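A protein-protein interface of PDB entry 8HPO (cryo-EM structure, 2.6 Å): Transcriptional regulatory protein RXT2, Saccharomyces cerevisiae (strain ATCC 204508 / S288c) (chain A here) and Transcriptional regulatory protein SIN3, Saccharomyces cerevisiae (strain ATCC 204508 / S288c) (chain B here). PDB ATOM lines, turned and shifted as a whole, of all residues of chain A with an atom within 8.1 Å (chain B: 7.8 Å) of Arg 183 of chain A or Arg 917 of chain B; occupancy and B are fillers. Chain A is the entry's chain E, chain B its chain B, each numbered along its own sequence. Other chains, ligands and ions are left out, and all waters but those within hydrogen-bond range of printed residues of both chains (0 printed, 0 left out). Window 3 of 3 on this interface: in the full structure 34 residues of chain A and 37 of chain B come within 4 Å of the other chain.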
ATOM      1  N   VAL A 160       4.585  -8.857  13.858  1.00  0.00           N
ATOM      2  CA  VAL A 160       3.429  -8.427  14.627  1.00  0.00           C
ATOM      3  C   VAL A 160       3.911  -7.439  15.678  1.00  0.00           C
ATOM      4  O   VAL A 160       4.682  -7.805  16.571  1.00  0.00           O
ATOM      5  CB  VAL A 160       2.720  -9.628  15.273  1.00  0.00           C
ATOM      6  CG1 VAL A 160       1.254  -9.357  15.444  1.00  0.00           C
ATOM      7  CG2 VAL A 160       2.929 -10.868  14.435  1.00  0.00           C
ATOM      8  N   ILE A 165      -1.072  -2.861  17.834  1.00  0.00           N
ATOM      9  CA  ILE A 165      -2.332  -3.596  17.876  1.00  0.00           C
ATOM     10  C   ILE A 165      -3.196  -3.116  19.035  1.00  0.00           C
ATOM     11  O   ILE A 165      -4.424  -3.037  18.927  1.00  0.00           O
ATOM     12  CB  ILE A 165      -2.057  -5.105  17.971  1.00  0.00           C
ATOM     13  CG1 ILE A 165      -1.401  -5.608  16.695  1.00  0.00           C
ATOM     14  CG2 ILE A 165      -3.327  -5.873  18.224  1.00  0.00           C
ATOM     15  CD1 ILE A 165      -0.968  -7.017  16.801  1.00  0.00           C
ATOM     16  N   ASP A 174      -9.201   6.661  12.530  1.00  0.00           N
ATOM     17  CA  ASP A 174      -8.638   5.373  12.908  1.00  0.00           C
ATOM     18  C   ASP A 174      -9.606   4.218  12.720  1.00  0.00           C
ATOM     19  O   ASP A 174      -9.222   3.069  12.942  1.00  0.00           O
ATOM     20  CB  ASP A 174      -8.166   5.409  14.359  1.00  0.00           C
ATOM     21  CG  ASP A 174      -7.122   6.469  14.596  1.00  0.00           C
ATOM     22  OD1 ASP A 174      -5.942   6.114  14.787  1.00  0.00           O
ATOM     23  OD2 ASP A 174      -7.483   7.662  14.583  1.00  0.00           O
ATOM     24  N   ILE A 175     -10.843   4.487  12.305  1.00  0.00           N
ATOM     25  CA  ILE A 175     -11.798   3.412  12.084  1.00  0.00           C
ATOM     26  C   ILE A 175     -11.509   2.678  10.779  1.00  0.00           C
ATOM     27  O   ILE A 175     -11.857   1.500  10.636  1.00  0.00           O
ATOM     28  CB  ILE A 175     -13.220   4.002  12.162  1.00  0.00           C
ATOM     29  CG1 ILE A 175     -13.581   4.262  13.619  1.00  0.00           C
ATOM     30  CG2 ILE A 175     -14.256   3.086  11.554  1.00  0.00           C
ATOM     31  CD1 ILE A 175     -14.237   5.576  13.835  1.00  0.00           C
ATOM     32  N   ILE A 176     -10.835   3.332   9.836  1.00  0.00           N
ATOM     33  CA  ILE A 176     -10.415   2.692   8.602  1.00  0.00           C
ATOM     34  C   ILE A 176      -8.902   2.509   8.522  1.00  0.00           C
ATOM     35  O   ILE A 176      -8.438   1.579   7.851  1.00  0.00           O
ATOM     36  CB  ILE A 176     -10.933   3.485   7.387  1.00  0.00           C
ATOM     37  CG1 ILE A 176     -10.831   4.979   7.658  1.00  0.00           C
ATOM     38  CG2 ILE A 176     -12.368   3.138   7.086  1.00  0.00           C
ATOM     39  CD1 ILE A 176     -11.518   5.795   6.629  1.00  0.00           C
ATOM     40  N   HIS A 178      -6.510   2.134  11.255  1.00  0.00           N
ATOM     41  CA  HIS A 178      -6.090   1.068  12.153  1.00  0.00           C
ATOM     42  C   HIS A 178      -6.454  -0.283  11.557  1.00  0.00           C
ATOM     43  O   HIS A 178      -7.458  -0.420  10.862  1.00  0.00           O
ATOM     44  CB  HIS A 178      -6.759   1.247  13.510  1.00  0.00           C
ATOM     45  CG  HIS A 178      -5.916   0.821  14.668  1.00  0.00           C
ATOM     46  ND1 HIS A 178      -5.662  -0.501  14.958  1.00  0.00           N
ATOM     47  CD2 HIS A 178      -5.289   1.543  15.623  1.00  0.00           C
ATOM     48  CE1 HIS A 178      -4.906  -0.572  16.036  1.00  0.00           C
ATOM     49  NE2 HIS A 178      -4.665   0.654  16.459  1.00  0.00           N
ATOM     50  N   LYS A 179      -5.628  -1.286  11.823  1.00  0.00           N
ATOM     51  CA  LYS A 179      -5.811  -2.559  11.141  1.00  0.00           C
ATOM     52  C   LYS A 179      -6.657  -3.529  11.952  1.00  0.00           C
ATOM     53  O   LYS A 179      -7.290  -4.419  11.376  1.00  0.00           O
ATOM     54  CB  LYS A 179      -4.451  -3.179  10.824  1.00  0.00           C
ATOM     55  CG  LYS A 179      -4.441  -4.056   9.591  1.00  0.00           C
ATOM     56  CD  LYS A 179      -4.646  -5.515   9.951  1.00  0.00           C
ATOM     57  CE  LYS A 179      -4.353  -6.427   8.772  1.00  0.00           C
ATOM     58  NZ  LYS A 179      -4.535  -7.859   9.127  1.00  0.00           N
ATOM     59  N   THR A 180      -6.678  -3.385  13.275  1.00  0.00           N
ATOM     60  CA  THR A 180      -7.583  -4.177  14.098  1.00  0.00           C
ATOM     61  C   THR A 180      -8.958  -3.534  14.197  1.00  0.00           C
ATOM     62  O   THR A 180      -9.972  -4.218  14.043  1.00  0.00           O
ATOM     63  CB  THR A 180      -7.004  -4.380  15.502  1.00  0.00           C
ATOM     64  OG1 THR A 180      -6.356  -3.182  15.938  1.00  0.00           O
ATOM     65  CG2 THR A 180      -6.005  -5.517  15.509  1.00  0.00           C
ATOM     66  N   ILE A 181      -9.004  -2.224  14.436  1.00  0.00           N
ATOM     67  CA  ILE A 181     -10.276  -1.535  14.613  1.00  0.00           C
ATOM     68  C   ILE A 181     -11.091  -1.541  13.327  1.00  0.00           C
ATOM     69  O   ILE A 181     -12.326  -1.563  13.368  1.00  0.00           O
ATOM     70  CB  ILE A 181     -10.011  -0.114  15.136  1.00  0.00           C
ATOM     71  CG1 ILE A 181      -9.667  -0.185  16.620  1.00  0.00           C
ATOM     72  CG2 ILE A 181     -11.202   0.782  14.908  1.00  0.00           C
ATOM     73  CD1 ILE A 181      -8.985   1.032  17.143  1.00  0.00           C
ATOM     74  N   SER A 182     -10.433  -1.559  12.172  1.00  0.00           N
ATOM     75  CA  SER A 182     -11.153  -1.655  10.911  1.00  0.00           C
ATOM     76  C   SER A 182     -11.789  -3.020  10.696  1.00  0.00           C
ATOM     77  O   SER A 182     -12.803  -3.106  10.002  1.00  0.00           O
ATOM     78  CB  SER A 182     -10.216  -1.344   9.748  1.00  0.00           C
ATOM     79  OG  SER A 182      -9.536  -2.509   9.326  1.00  0.00           O
ATOM     80  N   ARG A 183     -11.225  -4.076  11.271  1.00  0.00           N
ATOM     81  CA  ARG A 183     -11.778  -5.416  11.157  1.00  0.00           C
ATOM     82  C   ARG A 183     -13.109  -5.567  11.875  1.00  0.00           C
ATOM     83  O   ARG A 183     -13.801  -6.565  11.660  1.00  0.00           O
ATOM     84  CB  ARG A 183     -10.781  -6.431  11.709  1.00  0.00           C
ATOM     85  CG  ARG A 183     -10.874  -7.828  11.125  1.00  0.00           C
ATOM     86  CD  ARG A 183      -9.869  -8.729  11.823  1.00  0.00           C
ATOM     87  NE  ARG A 183      -9.677 -10.024  11.181  1.00  0.00           N
ATOM     88  CZ  ARG A 183     -10.508 -11.050  11.312  1.00  0.00           C
ATOM     89  NH1 ARG A 183     -11.599 -10.932  12.055  1.00  0.00           N
ATOM     90  NH2 ARG A 183     -10.249 -12.194  10.698  1.00  0.00           N
ATOM     91  N   THR A 184     -13.477  -4.609  12.724  1.00  0.00           N
ATOM     92  CA  THR A 184     -14.748  -4.633  13.427  1.00  0.00           C
ATOM     93  C   THR A 184     -15.827  -3.806  12.749  1.00  0.00           C
ATOM     94  O   THR A 184     -16.928  -4.319  12.541  1.00  0.00           O
ATOM     95  CB  THR A 184     -14.574  -4.122  14.866  1.00  0.00           C
ATOM     96  OG1 THR A 184     -13.759  -5.039  15.602  1.00  0.00           O
ATOM     97  CG2 THR A 184     -15.920  -3.983  15.556  1.00  0.00           C
ATOM     98  N   PHE A 185     -15.532  -2.565  12.378  1.00  0.00           N
ATOM     99  CA  PHE A 185     -16.514  -1.668  11.796  1.00  0.00           C
ATOM    100  C   PHE A 185     -16.830  -1.980  10.345  1.00  0.00           C
ATOM    101  O   PHE A 185     -17.486  -1.175   9.688  1.00  0.00           O
ATOM    102  CB  PHE A 185     -16.034  -0.227  11.895  1.00  0.00           C
ATOM    103  CG  PHE A 185     -16.257   0.391  13.227  1.00  0.00           C
ATOM    104  CD1 PHE A 185     -17.354   1.192  13.452  1.00  0.00           C
ATOM    105  CD2 PHE A 185     -15.356   0.187  14.253  1.00  0.00           C
ATOM    106  CE1 PHE A 185     -17.553   1.768  14.674  1.00  0.00           C
ATOM    107  CE2 PHE A 185     -15.553   0.762  15.474  1.00  0.00           C
ATOM    108  CZ  PHE A 185     -16.651   1.556  15.684  1.00  0.00           C
ATOM    109  N   SER A 186     -16.391  -3.122   9.828  1.00  0.00           N
ATOM    110  CA  SER A 186     -16.631  -3.487   8.442  1.00  0.00           C
ATOM    111  C   SER A 186     -17.052  -4.941   8.349  1.00  0.00           C
ATOM    112  O   SER A 186     -17.084  -5.529   7.265  1.00  0.00           O
ATOM    113  CB  SER A 186     -15.397  -3.234   7.584  1.00  0.00           C
ATOM    114  OG  SER A 186     -15.063  -1.859   7.571  1.00  0.00           O
ATOM    115  N   SER A 187     -17.382  -5.537   9.482  1.00  0.00           N
ATOM    116  CA  SER A 187     -17.779  -6.928   9.558  1.00  0.00           C
ATOM    117  C   SER A 187     -19.144  -7.130   8.914  1.00  0.00           C
ATOM    118  O   SER A 187     -20.070  -6.354   9.173  1.00  0.00           O
ATOM    119  CB  SER A 187     -17.837  -7.386  11.018  1.00  0.00           C
ATOM    120  OG  SER A 187     -16.893  -6.682  11.802  1.00  0.00           O
ATOM    121  N   PRO A 188     -19.296  -8.136   8.050  1.00  0.00           N
ATOM    122  CA  PRO A 188     -20.608  -8.479   7.492  1.00  0.00           C
ATOM    123  C   PRO A 188     -21.386  -9.461   8.363  1.00  0.00           C
ATOM    124  O   PRO A 188     -21.987 -10.420   7.869  1.00  0.00           O
ATOM    125  CB  PRO A 188     -20.236  -9.116   6.152  1.00  0.00           C
ATOM    126  CG  PRO A 188     -18.996  -9.869   6.504  1.00  0.00           C
ATOM    127  CD  PRO A 188     -18.239  -8.987   7.480  1.00  0.00           C
ATOM    128  N   ILE A 189     -21.393  -9.226   9.672  1.00  0.00           N
ATOM    129  CA  ILE A 189     -21.822 -10.229  10.631  1.00  0.00           C
ATOM    130  C   ILE A 189     -23.112  -9.832  11.338  1.00  0.00           C
ATOM    131  O   ILE A 189     -23.942 -10.691  11.639  1.00  0.00           O
ATOM    132  CB  ILE A 189     -20.693 -10.534  11.641  1.00  0.00           C
ATOM    133  CG1 ILE A 189     -20.568 -12.040  11.837  1.00  0.00           C
ATOM    134  CG2 ILE A 189     -20.912  -9.833  12.960  1.00  0.00           C
ATOM    135  CD1 ILE A 189     -19.982 -12.735  10.639  1.00  0.00           C
ATOM    136  N   ARG A 363     -23.263   1.027  13.705  1.00  0.00           N
ATOM    137  CA  ARG A 363     -21.999   0.667  13.069  1.00  0.00           C
ATOM    138  C   ARG A 363     -21.832   1.341  11.713  1.00  0.00           C
ATOM    139  O   ARG A 363     -20.790   1.955  11.440  1.00  0.00           O
ATOM    140  CB  ARG A 363     -21.931  -0.847  12.919  1.00  0.00           C
ATOM    141  CG  ARG A 363     -20.823  -1.357  12.056  1.00  0.00           C
ATOM    142  CD  ARG A 363     -21.171  -2.743  11.584  1.00  0.00           C
ATOM    143  NE  ARG A 363     -20.774  -2.986  10.202  1.00  0.00           N
ATOM    144  CZ  ARG A 363     -21.317  -2.399   9.140  1.00  0.00           C
ATOM    145  NH1 ARG A 363     -22.298  -1.522   9.274  1.00  0.00           N
ATOM    146  NH2 ARG A 363     -20.875  -2.700   7.932  1.00  0.00           N
ATOM    147  N   ILE B 810      -0.619 -21.196  20.359  1.00  0.00           N
ATOM    148  CA  ILE B 810      -1.786 -20.318  20.327  1.00  0.00           C
ATOM    149  C   ILE B 810      -3.056 -21.105  20.631  1.00  0.00           C
ATOM    150  O   ILE B 810      -3.924 -20.656  21.398  1.00  0.00           O
ATOM    151  CB  ILE B 810      -1.876 -19.616  18.964  1.00  0.00           C
ATOM    152  CG1 ILE B 810      -0.815 -18.531  18.857  1.00  0.00           C
ATOM    153  CG2 ILE B 810      -3.242 -19.004  18.768  1.00  0.00           C
ATOM    154  CD1 ILE B 810      -0.920 -17.750  17.586  1.00  0.00           C
ATOM    155  N   ARG B 814      -5.612 -20.311  23.931  1.00  0.00           N
ATOM    156  CA  ARG B 814      -7.024 -19.951  23.873  1.00  0.00           C
ATOM    157  C   ARG B 814      -7.901 -21.035  24.486  1.00  0.00           C
ATOM    158  O   ARG B 814      -8.946 -20.722  25.075  1.00  0.00           O
ATOM    159  CB  ARG B 814      -7.456 -19.617  22.441  1.00  0.00           C
ATOM    160  CG  ARG B 814      -7.230 -20.677  21.384  1.00  0.00           C
ATOM    161  CD  ARG B 814      -8.136 -20.435  20.168  1.00  0.00           C
ATOM    162  NE  ARG B 814      -7.739 -19.294  19.338  1.00  0.00           N
ATOM    163  CZ  ARG B 814      -8.383 -18.128  19.300  1.00  0.00           C
ATOM    164  NH1 ARG B 814      -9.455 -17.936  20.052  1.00  0.00           N
ATOM    165  NH2 ARG B 814      -7.962 -17.150  18.513  1.00  0.00           N
ATOM    166  N   ARG B 910     -11.249 -11.076  24.770  1.00  0.00           N
ATOM    167  CA  ARG B 910     -11.438 -10.299  23.546  1.00  0.00           C
ATOM    168  C   ARG B 910     -10.190  -9.486  23.204  1.00  0.00           C
ATOM    169  O   ARG B 910      -9.686  -9.520  22.062  1.00  0.00           O
ATOM    170  CB  ARG B 910     -12.647  -9.380  23.711  1.00  0.00           C
ATOM    171  CG  ARG B 910     -13.964  -9.999  23.300  1.00  0.00           C
ATOM    172  CD  ARG B 910     -15.127  -9.060  23.550  1.00  0.00           C
ATOM    173  NE  ARG B 910     -15.722  -9.282  24.861  1.00  0.00           N
ATOM    174  CZ  ARG B 910     -16.212  -8.317  25.625  1.00  0.00           C
ATOM    175  NH1 ARG B 910     -16.178  -7.064  25.207  1.00  0.00           N
ATOM    176  NH2 ARG B 910     -16.724  -8.603  26.809  1.00  0.00           N
ATOM    177  N   TRP B 912      -7.154  -9.897  23.983  1.00  0.00           N
ATOM    178  CA  TRP B 912      -6.025 -10.656  23.469  1.00  0.00           C
ATOM    179  C   TRP B 912      -6.349 -11.463  22.225  1.00  0.00           C
ATOM    180  O   TRP B 912      -5.424 -11.914  21.543  1.00  0.00           O
ATOM    181  CB  TRP B 912      -5.444 -11.592  24.528  1.00  0.00           C
ATOM    182  CG  TRP B 912      -3.999 -11.865  24.240  1.00  0.00           C
ATOM    183  CD1 TRP B 912      -3.465 -13.004  23.727  1.00  0.00           C
ATOM    184  CD2 TRP B 912      -2.913 -10.950  24.402  1.00  0.00           C
ATOM    185  NE1 TRP B 912      -2.113 -12.863  23.578  1.00  0.00           N
ATOM    186  CE2 TRP B 912      -1.750 -11.608  23.988  1.00  0.00           C
ATOM    187  CE3 TRP B 912      -2.812  -9.639  24.869  1.00  0.00           C
ATOM    188  CZ2 TRP B 912      -0.501 -11.006  24.030  1.00  0.00           C
ATOM    189  CZ3 TRP B 912      -1.575  -9.046  24.907  1.00  0.00           C
ATOM    190  CH2 TRP B 912      -0.437  -9.726  24.491  1.00  0.00           C
ATOM    191  N   ASN B 913      -7.622 -11.643  21.891  1.00  0.00           N
ATOM    192  CA  ASN B 913      -7.923 -12.245  20.603  1.00  0.00           C
ATOM    193  C   ASN B 913      -7.577 -11.297  19.474  1.00  0.00           C
ATOM    194  O   ASN B 913      -7.309 -11.742  18.358  1.00  0.00           O
ATOM    195  CB  ASN B 913      -9.391 -12.655  20.524  1.00  0.00           C
ATOM    196  CG  ASN B 913      -9.732 -13.326  19.218  1.00  0.00           C
ATOM    197  OD1 ASN B 913      -9.389 -14.485  18.990  1.00  0.00           O
ATOM    198  ND2 ASN B 913     -10.397 -12.596  18.340  1.00  0.00           N
ATOM    199  N   LYS B 914      -7.557  -9.992  19.744  1.00  0.00           N
ATOM    200  CA  LYS B 914      -7.002  -9.074  18.744  1.00  0.00           C
ATOM    201  C   LYS B 914      -5.586  -9.484  18.319  1.00  0.00           C
ATOM    202  O   LYS B 914      -5.296  -9.641  17.121  1.00  0.00           O
ATOM    203  CB  LYS B 914      -7.013  -7.643  19.273  1.00  0.00           C
ATOM    204  CG  LYS B 914      -8.350  -6.978  19.111  1.00  0.00           C
ATOM    205  CD  LYS B 914      -8.298  -5.514  19.432  1.00  0.00           C
ATOM    206  CE  LYS B 914      -7.917  -5.282  20.867  1.00  0.00           C
ATOM    207  NZ  LYS B 914      -8.680  -4.157  21.455  1.00  0.00           N
ATOM    208  N   VAL B 915      -4.688  -9.665  19.291  1.00  0.00           N
ATOM    209  CA  VAL B 915      -3.324 -10.104  19.002  1.00  0.00           C
ATOM    210  C   VAL B 915      -3.310 -11.500  18.399  1.00  0.00           C
ATOM    211  O   VAL B 915      -2.594 -11.758  17.427  1.00  0.00           O
ATOM    212  CB  VAL B 915      -2.464 -10.041  20.273  1.00  0.00           C
ATOM    213  CG1 VAL B 915      -1.090 -10.590  19.999  1.00  0.00           C
ATOM    214  CG2 VAL B 915      -2.378  -8.623  20.779  1.00  0.00           C
ATOM    215  N   TRP B 916      -4.059 -12.433  18.992  1.00  0.00           N
ATOM    216  CA  TRP B 916      -4.149 -13.785  18.448  1.00  0.00           C
ATOM    217  C   TRP B 916      -4.555 -13.788  16.983  1.00  0.00           C
ATOM    218  O   TRP B 916      -4.152 -14.678  16.227  1.00  0.00           O
ATOM    219  CB  TRP B 916      -5.173 -14.597  19.234  1.00  0.00           C
ATOM    220  CG  TRP B 916      -4.663 -15.327  20.416  1.00  0.00           C
ATOM    221  CD1 TRP B 916      -3.414 -15.833  20.601  1.00  0.00           C
ATOM    222  CD2 TRP B 916      -5.406 -15.651  21.590  1.00  0.00           C
ATOM    223  NE1 TRP B 916      -3.331 -16.445  21.824  1.00  0.00           N
ATOM    224  CE2 TRP B 916      -4.543 -16.345  22.451  1.00  0.00           C
ATOM    225  CE3 TRP B 916      -6.717 -15.407  22.001  1.00  0.00           C
ATOM    226  CZ2 TRP B 916      -4.949 -16.803  23.694  1.00  0.00           C
ATOM    227  CZ3 TRP B 916      -7.116 -15.859  23.233  1.00  0.00           C
ATOM    228  CH2 TRP B 916      -6.237 -16.551  24.066  1.00  0.00           C
ATOM    229  N   ARG B 917      -5.371 -12.819  16.571  1.00  0.00           N
ATOM    230  CA  ARG B 917      -5.888 -12.778  15.211  1.00  0.00           C
ATOM    231  C   ARG B 917      -4.868 -12.178  14.263  1.00  0.00           C
ATOM    232  O   ARG B 917      -4.636 -12.709  13.172  1.00  0.00           O
ATOM    233  CB  ARG B 917      -7.183 -11.967  15.171  1.00  0.00           C
ATOM    234  CG  ARG B 917      -8.317 -12.626  14.424  1.00  0.00           C
ATOM    235  CD  ARG B 917      -9.637 -12.148  14.982  1.00  0.00           C
ATOM    236  NE  ARG B 917      -9.580 -10.731  15.317  1.00  0.00           N
ATOM    237  CZ  ARG B 917     -10.644  -9.981  15.573  1.00  0.00           C
ATOM    238  NH1 ARG B 917     -11.856 -10.514  15.530  1.00  0.00           N
ATOM    239  NH2 ARG B 917     -10.494  -8.697  15.868  1.00  0.00           N
ATOM    240  N   GLU B 918      -4.257 -11.060  14.657  1.00  0.00           N
ATOM    241  CA  GLU B 918      -3.203 -10.484  13.830  1.00  0.00           C
ATOM    242  C   GLU B 918      -1.992 -11.397  13.712  1.00  0.00           C
ATOM    243  O   GLU B 918      -1.250 -11.296  12.733  1.00  0.00           O
ATOM    244  CB  GLU B 918      -2.780  -9.136  14.394  1.00  0.00           C
ATOM    245  CG  GLU B 918      -1.873  -8.352  13.490  1.00  0.00           C
ATOM    246  CD  GLU B 918      -2.459  -7.007  13.118  1.00  0.00           C
ATOM    247  OE1 GLU B 918      -1.683  -6.082  12.797  1.00  0.00           O
ATOM    248  OE2 GLU B 918      -3.700  -6.880  13.142  1.00  0.00           O
ATOM    249  N   LEU B 919      -1.798 -12.294  14.668  1.00  0.00           N
ATOM    250  CA  LEU B 919      -0.653 -13.185  14.737  1.00  0.00           C
ATOM    251  C   LEU B 919      -0.832 -14.464  13.930  1.00  0.00           C
ATOM    252  O   LEU B 919       0.083 -15.289  13.892  1.00  0.00           O
ATOM    253  CB  LEU B 919      -0.395 -13.513  16.212  1.00  0.00           C
ATOM    254  CG  LEU B 919       0.794 -14.290  16.755  1.00  0.00           C
ATOM    255  CD1 LEU B 919       2.040 -13.465  16.664  1.00  0.00           C
ATOM    256  CD2 LEU B 919       0.506 -14.609  18.195  1.00  0.00           C
ATOM    257  N   GLU B 920      -1.976 -14.651  13.279  1.00  0.00           N
ATOM    258  CA  GLU B 920      -2.268 -15.909  12.605  1.00  0.00           C
ATOM    259  C   GLU B 920      -2.239 -15.809  11.088  1.00  0.00           C
ATOM    260  O   GLU B 920      -1.913 -16.801  10.430  1.00  0.00           O
ATOM    261  CB  GLU B 920      -3.638 -16.441  13.041  1.00  0.00           C
ATOM    262  CG  GLU B 920      -3.597 -17.780  13.758  1.00  0.00           C
ATOM    263  CD  GLU B 920      -3.576 -18.959  12.809  1.00  0.00           C
ATOM    264  OE1 GLU B 920      -3.408 -18.746  11.595  1.00  0.00           O
ATOM    265  OE2 GLU B 920      -3.734 -20.104  13.279  1.00  0.00           O
ATOM    266  N   GLN B 921      -2.577 -14.653  10.517  1.00  0.00           N
ATOM    267  CA  GLN B 921      -2.434 -14.489   9.074  1.00  0.00           C
ATOM    268  C   GLN B 921      -0.987 -14.670   8.642  1.00  0.00           C
ATOM    269  O   GLN B 921      -0.712 -15.288   7.608  1.00  0.00           O
ATOM    270  CB  GLN B 921      -2.934 -13.115   8.640  1.00  0.00           C
ATOM    271  CG  GLN B 921      -4.195 -12.661   9.306  1.00  0.00           C
ATOM    272  CD  GLN B 921      -4.101 -11.221   9.736  1.00  0.00           C
ATOM    273  OE1 GLN B 921      -3.022 -10.632   9.724  1.00  0.00           O
ATOM    274  NE2 GLN B 921      -5.230 -10.638  10.118  1.00  0.00           N
ATOM    275  N   LYS B 922      -0.052 -14.135   9.427  1.00  0.00           N
ATOM    276  CA  LYS B 922       1.359 -14.198   9.070  1.00  0.00           C
ATOM    277  C   LYS B 922       1.901 -15.613   9.186  1.00  0.00           C
ATOM    278  O   LYS B 922       2.616 -16.085   8.299  1.00  0.00           O
ATOM    279  CB  LYS B 922       2.158 -13.258   9.963  1.00  0.00           C
ATOM    280  CG  LYS B 922       2.202 -11.828   9.482  1.00  0.00           C
ATOM    281  CD  LYS B 922       0.916 -11.099   9.790  1.00  0.00           C
ATOM    282  CE  LYS B 922       1.162  -9.622  10.015  1.00  0.00           C
ATOM    283  NZ  LYS B 922       1.924  -9.012   8.888  1.00  0.00           N
ATOM    284  N   VAL B 923       1.562 -16.308  10.265  1.00  0.00           N
ATOM    285  CA  VAL B 923       2.257 -17.542  10.595  1.00  0.00           C
ATOM    286  C   VAL B 923       1.661 -18.747   9.870  1.00  0.00           C
ATOM    287  O   VAL B 923       2.357 -19.743   9.646  1.00  0.00           O
ATOM    288  CB  VAL B 923       2.239 -17.717  12.122  1.00  0.00           C
ATOM    289  CG1 VAL B 923       2.905 -19.000  12.537  1.00  0.00           C
ATOM    290  CG2 VAL B 923       2.924 -16.542  12.780  1.00  0.00           C
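Along chain A the printed residues that touch a printed residue of chain B span positions 160 to 183. Printed residues of chain B that touch a printed residue of chain A: Val 915, Arg 917, Glu 918, Leu 919 and Gln 921. Hydrophobic or aromatic side chains of chain B that line the printed part of chain A: Val 915 and Leu 919.
Of the printed residues of chain B, Lys 179 of chain A touches Glu 918 (3.6 Å) and Gln 921 (3.0 Å). Printed residues of chain B within 4 Å of Thr 180 of chain A: Glu 918. No residue of chain B comes within 4 Å of Ser 182 of chain A. Printed residues of chain A within 4 Å of Val 915 of chain B: Ile 165 (3.9 Å). Of chain A, only Arg 183 (3.5 Å) comes within 4 Å of Arg 917 of chain B. Printed residues of chain A within 4 Å of Glu 918 of chain B: Val 160, Ile 165, Lys 179 and Thr 180. Printed residues of chain A within 4 Å of Leu 919 of chain B: Val 160. The nearest printed residue of chain A that does not touch Glu 918 of chain B is Arg 183 of chain A (6.5 Å).
The side-chain amino group (NZ) of Lys 179 of chain A lies close to the side-chain amide nitrogen (NE2) of Gln 921 of chain B.
A ring nitrogen (ND1) of His 178 of chain A lies within hydrogen-bond range of the side-chain hydroxyl (OG1) of Thr 180 of chain A. O of Arg 183 of chain A lies within hydrogen-bond range of OG of Ser 187 of chain A (3.1 Å).
CG of Glu 918 of chain B touches CG1 of Val 160 of chain A (3.8 Å). Leu 919 of chain B touches Val 160 of chain A. Ile 165 of chain A touches Val 915 of chain B. CG of Glu 918 of chain B touches CD1 of Ile 165 of chain A (3.7 Å). Lys 179 of chain A touches Glu 918 of chain B (CD to OE2, 3.6 Å). OE2 of Glu 918 of chain B touches CG2 of Thr 180 of chain A (3.6 Å). NH1 of Arg 917 of chain B touches NH1 of Arg 183 of chain A, at 3.5 Å.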
